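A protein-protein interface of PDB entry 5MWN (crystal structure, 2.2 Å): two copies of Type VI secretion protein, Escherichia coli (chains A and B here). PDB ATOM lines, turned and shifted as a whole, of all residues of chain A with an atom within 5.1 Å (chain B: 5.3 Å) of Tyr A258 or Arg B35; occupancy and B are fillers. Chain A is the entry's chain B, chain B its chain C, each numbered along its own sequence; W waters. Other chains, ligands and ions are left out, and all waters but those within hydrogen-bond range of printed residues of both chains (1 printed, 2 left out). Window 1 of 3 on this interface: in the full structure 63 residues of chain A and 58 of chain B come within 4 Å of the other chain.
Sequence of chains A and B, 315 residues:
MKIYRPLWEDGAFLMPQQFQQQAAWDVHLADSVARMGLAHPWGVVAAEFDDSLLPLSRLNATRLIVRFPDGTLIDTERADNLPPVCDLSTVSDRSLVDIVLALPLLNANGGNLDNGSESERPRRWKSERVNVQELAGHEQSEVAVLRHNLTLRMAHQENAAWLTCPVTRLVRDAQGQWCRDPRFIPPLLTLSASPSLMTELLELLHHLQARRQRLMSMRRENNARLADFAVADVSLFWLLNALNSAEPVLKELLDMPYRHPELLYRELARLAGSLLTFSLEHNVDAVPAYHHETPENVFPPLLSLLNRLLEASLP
N of His A260 lies within hydrogen-bond range of O of Met B36, at 2.8 Å.
O of Tyr A258 sits close to O of Arg B35 (3.2 Å).
O of Leu A189 sits at hydrogen-bond distance from N of His A260 (3.4 Å).
OG1 of Thr A190 lies close to O of Tyr A258.
The backbone carbonyl oxygen (O) of Met A256 lies within hydrogen-bond range of the guanidinium group (NH2) of Arg A259 (2.8 Å).
OD2 of Asp B31 is in salt-bridge range of NE of Arg B35, 2.8 Å away.
The guanidinium group (NH2) of Arg B35 is in hydrogen-bond range of the backbone carbonyl oxygen (O) of Pro B69 (3.5 Å).
Among the printed residues, pairs that only touch across the chains: Arg A259 with Gly B37, Arg A259 with Met B36, Arg A259 with Ala B39, Arg A259 with Leu B38, Met A256 with Ala B39, Leu A189 with Met B36 and Arg A259 with Arg B35.
Of the printed residues of chain B, Met A256 touches Ala B39.
Of chain B, only Arg B35 (3.2 Å) comes within 4 Å of Tyr A258.
Of chain A, only Tyr A258 (3.2 Å) and Arg A259 (3.9 Å) come within 4 Å of Arg B35.
Of the printed residues of chain A, Met B36 touches Leu A189 (3.9 Å), Arg A259 (3.5 Å) and His A260 (2.8 Å).
Printed residues of chain A within 4 Å of Gly B37: Arg A259.
Of the printed residues of chain A, Leu B38 touches Arg A259.
Pro B41 touches none of the printed residues of chain A.
Pro B69 touches none of the printed residues of chain A.
The nearest residue of chain B that does not touch Tyr A258 is Met B36 (5.1 Å).
Of the 12 printed residues of chain B, 5 touch a printed residue of chain A.
Hydrophobic or aromatic side chains of chain B that line the printed part of chain A: Met B36 and Ala B39.
Along chain A the printed residues that touch a printed residue of chain B span positions 189 to 260.
No position is printed for both chains.
Of the 9 pairs that touch across the chains among the printed residues, none has its exchanged pair printed and touching as well.
Water W1 bridges O of Gly B37 (2.9 Å) and NH1 of Arg A259 (3.1 Å).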
ATOM      1  N   LEU A 189      27.403   7.036 -13.439  1.00  0.00           N
ATOM      2  CA  LEU A 189      27.134   8.467 -13.557  1.00  0.00           C
ATOM      3  C   LEU A 189      25.641   8.600 -13.831  1.00  0.00           C
ATOM      4  O   LEU A 189      25.056   9.652 -13.618  1.00  0.00           O
ATOM      5  CB  LEU A 189      27.934   9.113 -14.695  1.00  0.00           C
ATOM      6  CG  LEU A 189      29.059  10.075 -14.309  1.00  0.00           C
ATOM      7  CD1 LEU A 189      29.472  10.885 -15.500  1.00  0.00           C
ATOM      8  CD2 LEU A 189      28.641  11.041 -13.200  1.00  0.00           C
ATOM      9  N   THR A 190      25.036   7.508 -14.308  1.00  0.00           N
ATOM     10  CA  THR A 190      23.614   7.367 -14.617  1.00  0.00           C
ATOM     11  C   THR A 190      23.201   5.939 -14.264  1.00  0.00           C
ATOM     12  O   THR A 190      24.033   5.035 -14.356  1.00  0.00           O
ATOM     13  CB  THR A 190      23.311   7.760 -16.090  1.00  0.00           C
ATOM     14  OG1 THR A 190      21.938   7.518 -16.366  1.00  0.00           O
ATOM     15  CG2 THR A 190      24.113   6.976 -17.087  1.00  0.00           C
ATOM     16  N   LEU A 191      21.942   5.734 -13.840  1.00  0.00           N
ATOM     17  CA  LEU A 191      21.427   4.405 -13.494  1.00  0.00           C
ATOM     18  C   LEU A 191      21.254   3.549 -14.754  1.00  0.00           C
ATOM     19  O   LEU A 191      21.469   2.339 -14.707  1.00  0.00           O
ATOM     20  CB  LEU A 191      20.083   4.482 -12.733  1.00  0.00           C
ATOM     21  CG  LEU A 191      19.968   5.391 -11.490  1.00  0.00           C
ATOM     22  CD1 LEU A 191      18.561   5.323 -10.905  1.00  0.00           C
ATOM     23  CD2 LEU A 191      21.000   5.033 -10.423  1.00  0.00           C
ATOM     24  N   SER A 192      20.873   4.188 -15.879  1.00  0.00           N
ATOM     25  CA  SER A 192      20.633   3.561 -17.183  1.00  0.00           C
ATOM     26  C   SER A 192      21.856   2.846 -17.765  1.00  0.00           C
ATOM     27  O   SER A 192      21.689   1.961 -18.606  1.00  0.00           O
ATOM     28  CB  SER A 192      20.079   4.580 -18.175  1.00  0.00           C
ATOM     29  OG  SER A 192      20.918   5.719 -18.281  1.00  0.00           O
ATOM     30  N   LEU A 253      12.731   8.831  -9.377  1.00  0.00           N
ATOM     31  CA  LEU A 253      14.151   8.568  -9.647  1.00  0.00           C
ATOM     32  C   LEU A 253      14.329   7.474 -10.698  1.00  0.00           C
ATOM     33  O   LEU A 253      15.264   7.524 -11.500  1.00  0.00           O
ATOM     34  CB  LEU A 253      14.919   8.190  -8.373  1.00  0.00           C
ATOM     35  CG  LEU A 253      15.151   9.298  -7.355  1.00  0.00           C
ATOM     36  CD1 LEU A 253      15.685   8.735  -6.073  1.00  0.00           C
ATOM     37  CD2 LEU A 253      16.077  10.383  -7.901  1.00  0.00           C
ATOM     38  N   MET A 256      12.873   8.413 -14.710  1.00  0.00           N
ATOM     39  CA  MET A 256      13.894   9.140 -15.478  1.00  0.00           C
ATOM     40  C   MET A 256      15.237   8.760 -14.838  1.00  0.00           C
ATOM     41  O   MET A 256      15.758   9.490 -14.001  1.00  0.00           O
ATOM     42  CB  MET A 256      13.631  10.652 -15.474  1.00  0.00           C
ATOM     43  CG  MET A 256      12.444  11.057 -16.335  1.00  0.00           C
ATOM     44  SD  MET A 256      12.649  10.736 -18.118  1.00  0.00           S
ATOM     45  CE  MET A 256      13.804  12.017 -18.567  1.00  0.00           C
ATOM     46  N   PRO A 257      15.753   7.548 -15.146  1.00  0.00           N
ATOM     47  CA  PRO A 257      16.945   7.057 -14.444  1.00  0.00           C
ATOM     48  C   PRO A 257      18.264   7.499 -15.051  1.00  0.00           C
ATOM     49  O   PRO A 257      19.138   6.675 -15.299  1.00  0.00           O
ATOM     50  CB  PRO A 257      16.752   5.546 -14.506  1.00  0.00           C
ATOM     51  CG  PRO A 257      16.081   5.327 -15.830  1.00  0.00           C
ATOM     52  CD  PRO A 257      15.247   6.534 -16.104  1.00  0.00           C
ATOM     53  N   TYR A 258      18.423   8.811 -15.232  1.00  0.00           N
ATOM     54  CA  TYR A 258      19.597   9.373 -15.877  1.00  0.00           C
ATOM     55  C   TYR A 258      20.492  10.191 -14.946  1.00  0.00           C
ATOM     56  O   TYR A 258      21.451  10.812 -15.403  1.00  0.00           O
ATOM     57  CB  TYR A 258      19.154  10.165 -17.122  1.00  0.00           C
ATOM     58  CG  TYR A 258      18.250   9.338 -18.014  1.00  0.00           C
ATOM     59  CD1 TYR A 258      18.720   8.191 -18.646  1.00  0.00           C
ATOM     60  CD2 TYR A 258      16.904   9.661 -18.166  1.00  0.00           C
ATOM     61  CE1 TYR A 258      17.884   7.403 -19.434  1.00  0.00           C
ATOM     62  CE2 TYR A 258      16.059   8.888 -18.962  1.00  0.00           C
ATOM     63  CZ  TYR A 258      16.555   7.758 -19.594  1.00  0.00           C
ATOM     64  OH  TYR A 258      15.731   6.985 -20.376  1.00  0.00           O
ATOM     65  N   ARG A 259      20.214  10.133 -13.633  1.00  0.00           N
ATOM     66  CA  ARG A 259      20.976  10.856 -12.607  1.00  0.00           C
ATOM     67  C   ARG A 259      21.967   9.947 -11.875  1.00  0.00           C
ATOM     68  O   ARG A 259      21.876   8.721 -11.958  1.00  0.00           O
ATOM     69  CB  ARG A 259      20.037  11.560 -11.610  1.00  0.00           C
ATOM     70  CG  ARG A 259      19.272  12.728 -12.207  1.00  0.00           C
ATOM     71  CD  ARG A 259      17.980  12.981 -11.462  1.00  0.00           C
ATOM     72  NE  ARG A 259      16.984  11.941 -11.732  1.00  0.00           N
ATOM     73  CZ  ARG A 259      15.679  12.091 -11.557  1.00  0.00           C
ATOM     74  NH1 ARG A 259      15.189  13.244 -11.119  1.00  0.00           N
ATOM     75  NH2 ARG A 259      14.847  11.101 -11.847  1.00  0.00           N
ATOM     76  N   HIS A 260      22.906  10.572 -11.149  1.00  0.00           N
ATOM     77  CA  HIS A 260      23.955   9.942 -10.359  1.00  0.00           C
ATOM     78  C   HIS A 260      23.384   8.981  -9.288  1.00  0.00           C
ATOM     79  O   HIS A 260      22.361   9.295  -8.664  1.00  0.00           O
ATOM     80  CB  HIS A 260      24.798  11.045  -9.701  1.00  0.00           C
ATOM     81  CG  HIS A 260      26.148  10.602  -9.245  1.00  0.00           C
ATOM     82  ND1 HIS A 260      26.319   9.905  -8.066  1.00  0.00           N
ATOM     83  CD2 HIS A 260      27.356  10.804  -9.810  1.00  0.00           C
ATOM     84  CE1 HIS A 260      27.613   9.678  -7.969  1.00  0.00           C
ATOM     85  NE2 HIS A 260      28.277  10.213  -8.988  1.00  0.00           N
ATOM     86  N   ASP B  31      26.314  20.915 -19.766  1.00  0.00           N
ATOM     87  CA  ASP B  31      25.057  20.166 -19.819  1.00  0.00           C
ATOM     88  C   ASP B  31      25.192  18.770 -19.178  1.00  0.00           C
ATOM     89  O   ASP B  31      24.274  18.323 -18.502  1.00  0.00           O
ATOM     90  CB  ASP B  31      24.551  20.044 -21.269  1.00  0.00           C
ATOM     91  CG  ASP B  31      23.167  19.427 -21.380  1.00  0.00           C
ATOM     92  OD1 ASP B  31      22.184  20.090 -20.987  1.00  0.00           O
ATOM     93  OD2 ASP B  31      23.069  18.281 -21.846  1.00  0.00           O
ATOM     94  N   SER B  32      26.344  18.102 -19.368  1.00  0.00           N
ATOM     95  CA  SER B  32      26.580  16.766 -18.818  1.00  0.00           C
ATOM     96  C   SER B  32      26.680  16.814 -17.292  1.00  0.00           C
ATOM     97  O   SER B  32      26.251  15.872 -16.624  1.00  0.00           O
ATOM     98  CB  SER B  32      27.805  16.118 -19.455  1.00  0.00           C
ATOM     99  OG  SER B  32      29.006  16.765 -19.070  1.00  0.00           O
ATOM    100  N   VAL B  33      27.186  17.940 -16.743  1.00  0.00           N
ATOM    101  CA  VAL B  33      27.293  18.172 -15.299  1.00  0.00           C
ATOM    102  C   VAL B  33      25.874  18.370 -14.736  1.00  0.00           C
ATOM    103  O   VAL B  33      25.524  17.766 -13.723  1.00  0.00           O
ATOM    104  CB  VAL B  33      28.242  19.354 -14.967  1.00  0.00           C
ATOM    105  CG1 VAL B  33      28.133  19.776 -13.502  1.00  0.00           C
ATOM    106  CG2 VAL B  33      29.687  19.023 -15.325  1.00  0.00           C
ATOM    107  N   ALA B  34      25.052  19.172 -15.419  1.00  0.00           N
ATOM    108  CA  ALA B  34      23.665  19.416 -15.020  1.00  0.00           C
ATOM    109  C   ALA B  34      22.851  18.108 -14.960  1.00  0.00           C
ATOM    110  O   ALA B  34      22.024  17.948 -14.061  1.00  0.00           O
ATOM    111  CB  ALA B  34      23.019  20.401 -15.984  1.00  0.00           C
ATOM    112  N   ARG B  35      23.114  17.171 -15.904  1.00  0.00           N
ATOM    113  CA  ARG B  35      22.424  15.884 -16.009  1.00  0.00           C
ATOM    114  C   ARG B  35      22.781  14.894 -14.904  1.00  0.00           C
ATOM    115  O   ARG B  35      22.058  13.924 -14.713  1.00  0.00           O
ATOM    116  CB  ARG B  35      22.625  15.258 -17.395  1.00  0.00           C
ATOM    117  CG  ARG B  35      21.853  16.028 -18.442  1.00  0.00           C
ATOM    118  CD  ARG B  35      22.017  15.521 -19.862  1.00  0.00           C
ATOM    119  NE  ARG B  35      21.304  16.413 -20.777  1.00  0.00           N
ATOM    120  CZ  ARG B  35      19.996  16.358 -21.018  1.00  0.00           C
ATOM    121  NH1 ARG B  35      19.246  15.421 -20.450  1.00  0.00           N
ATOM    122  NH2 ARG B  35      19.431  17.236 -21.831  1.00  0.00           N
ATOM    123  N   MET B  36      23.879  15.134 -14.172  1.00  0.00           N
ATOM    124  CA  MET B  36      24.288  14.275 -13.060  1.00  0.00           C
ATOM    125  C   MET B  36      23.291  14.365 -11.903  1.00  0.00           C
ATOM    126  O   MET B  36      23.031  13.365 -11.244  1.00  0.00           O
ATOM    127  CB  MET B  36      25.688  14.665 -12.554  1.00  0.00           C
ATOM    128  CG  MET B  36      26.792  14.467 -13.564  1.00  0.00           C
ATOM    129  SD  MET B  36      28.387  14.877 -12.832  1.00  0.00           S
ATOM    130  CE  MET B  36      29.392  14.891 -14.273  1.00  0.00           C
ATOM    131  N   GLY B  37      22.762  15.562 -11.656  1.00  0.00           N
ATOM    132  CA  GLY B  37      21.832  15.802 -10.557  1.00  0.00           C
ATOM    133  C   GLY B  37      20.392  15.968 -10.984  1.00  0.00           C
ATOM    134  O   GLY B  37      19.482  15.772 -10.176  1.00  0.00           O
ATOM    135  N   LEU B  38      20.165  16.339 -12.253  1.00  0.00           N
ATOM    136  CA  LEU B  38      18.801  16.587 -12.741  1.00  0.00           C
ATOM    137  C   LEU B  38      18.464  15.852 -14.012  1.00  0.00           C
ATOM    138  O   LEU B  38      19.294  15.749 -14.919  1.00  0.00           O
ATOM    139  CB  LEU B  38      18.551  18.093 -12.905  1.00  0.00           C
ATOM    140  CG  LEU B  38      18.824  18.951 -11.659  1.00  0.00           C
ATOM    141  CD1 LEU B  38      19.203  20.342 -12.046  1.00  0.00           C
ATOM    142  CD2 LEU B  38      17.664  18.901 -10.659  1.00  0.00           C
ATOM    143  N   ALA B  39      17.233  15.351 -14.081  1.00  0.00           N
ATOM    144  CA  ALA B  39      16.728  14.602 -15.230  1.00  0.00           C
ATOM    145  C   ALA B  39      16.377  15.526 -16.390  1.00  0.00           C
ATOM    146  O   ALA B  39      16.515  15.134 -17.543  1.00  0.00           O
ATOM    147  CB  ALA B  39      15.505  13.792 -14.819  1.00  0.00           C
ATOM    148  N   PRO B  41      17.468  19.183 -17.290  1.00  0.00           N
ATOM    149  CA  PRO B  41      18.127  20.488 -17.123  1.00  0.00           C
ATOM    150  C   PRO B  41      17.841  21.474 -18.261  1.00  0.00           C
ATOM    151  O   PRO B  41      18.734  21.844 -19.022  1.00  0.00           O
ATOM    152  CB  PRO B  41      19.607  20.108 -17.025  1.00  0.00           C
ATOM    153  CG  PRO B  41      19.725  18.919 -17.899  1.00  0.00           C
ATOM    154  CD  PRO B  41      18.427  18.161 -17.763  1.00  0.00           C
ATOM    155  N   TRP B  42      16.580  21.882 -18.388  1.00  0.00           N
ATOM    156  CA  TRP B  42      16.146  22.834 -19.399  1.00  0.00           C
ATOM    157  C   TRP B  42      14.835  23.436 -18.920  1.00  0.00           C
ATOM    158  O   TRP B  42      14.188  22.873 -18.032  1.00  0.00           O
ATOM    159  CB  TRP B  42      16.016  22.178 -20.799  1.00  0.00           C
ATOM    160  CG  TRP B  42      14.998  21.088 -20.867  1.00  0.00           C
ATOM    161  CD1 TRP B  42      15.197  19.761 -20.621  1.00  0.00           C
ATOM    162  CD2 TRP B  42      13.617  21.230 -21.215  1.00  0.00           C
ATOM    163  NE1 TRP B  42      14.027  19.066 -20.801  1.00  0.00           N
ATOM    164  CE2 TRP B  42      13.039  19.943 -21.166  1.00  0.00           C
ATOM    165  CE3 TRP B  42      12.814  22.320 -21.597  1.00  0.00           C
ATOM    166  CZ2 TRP B  42      11.696  19.717 -21.465  1.00  0.00           C
ATOM    167  CZ3 TRP B  42      11.481  22.092 -21.912  1.00  0.00           C
ATOM    168  CH2 TRP B  42      10.934  20.803 -21.836  1.00  0.00           C
ATOM    169  N   PRO B  69      16.664  22.187 -24.548  1.00  0.00           N
ATOM    170  CA  PRO B  69      17.175  20.824 -24.256  1.00  0.00           C
ATOM    171  C   PRO B  69      18.521  20.446 -24.881  1.00  0.00           C
ATOM    172  O   PRO B  69      19.100  19.433 -24.474  1.00  0.00           O
ATOM    173  CB  PRO B  69      16.061  19.887 -24.738  1.00  0.00           C
ATOM    174  CG  PRO B  69      14.922  20.735 -25.100  1.00  0.00           C
ATOM    175  CD  PRO B  69      15.354  22.147 -25.233  1.00  0.00           C
HETATM  176  O   HOH W   1      16.668  15.498  -9.658  1.00  0.00           O
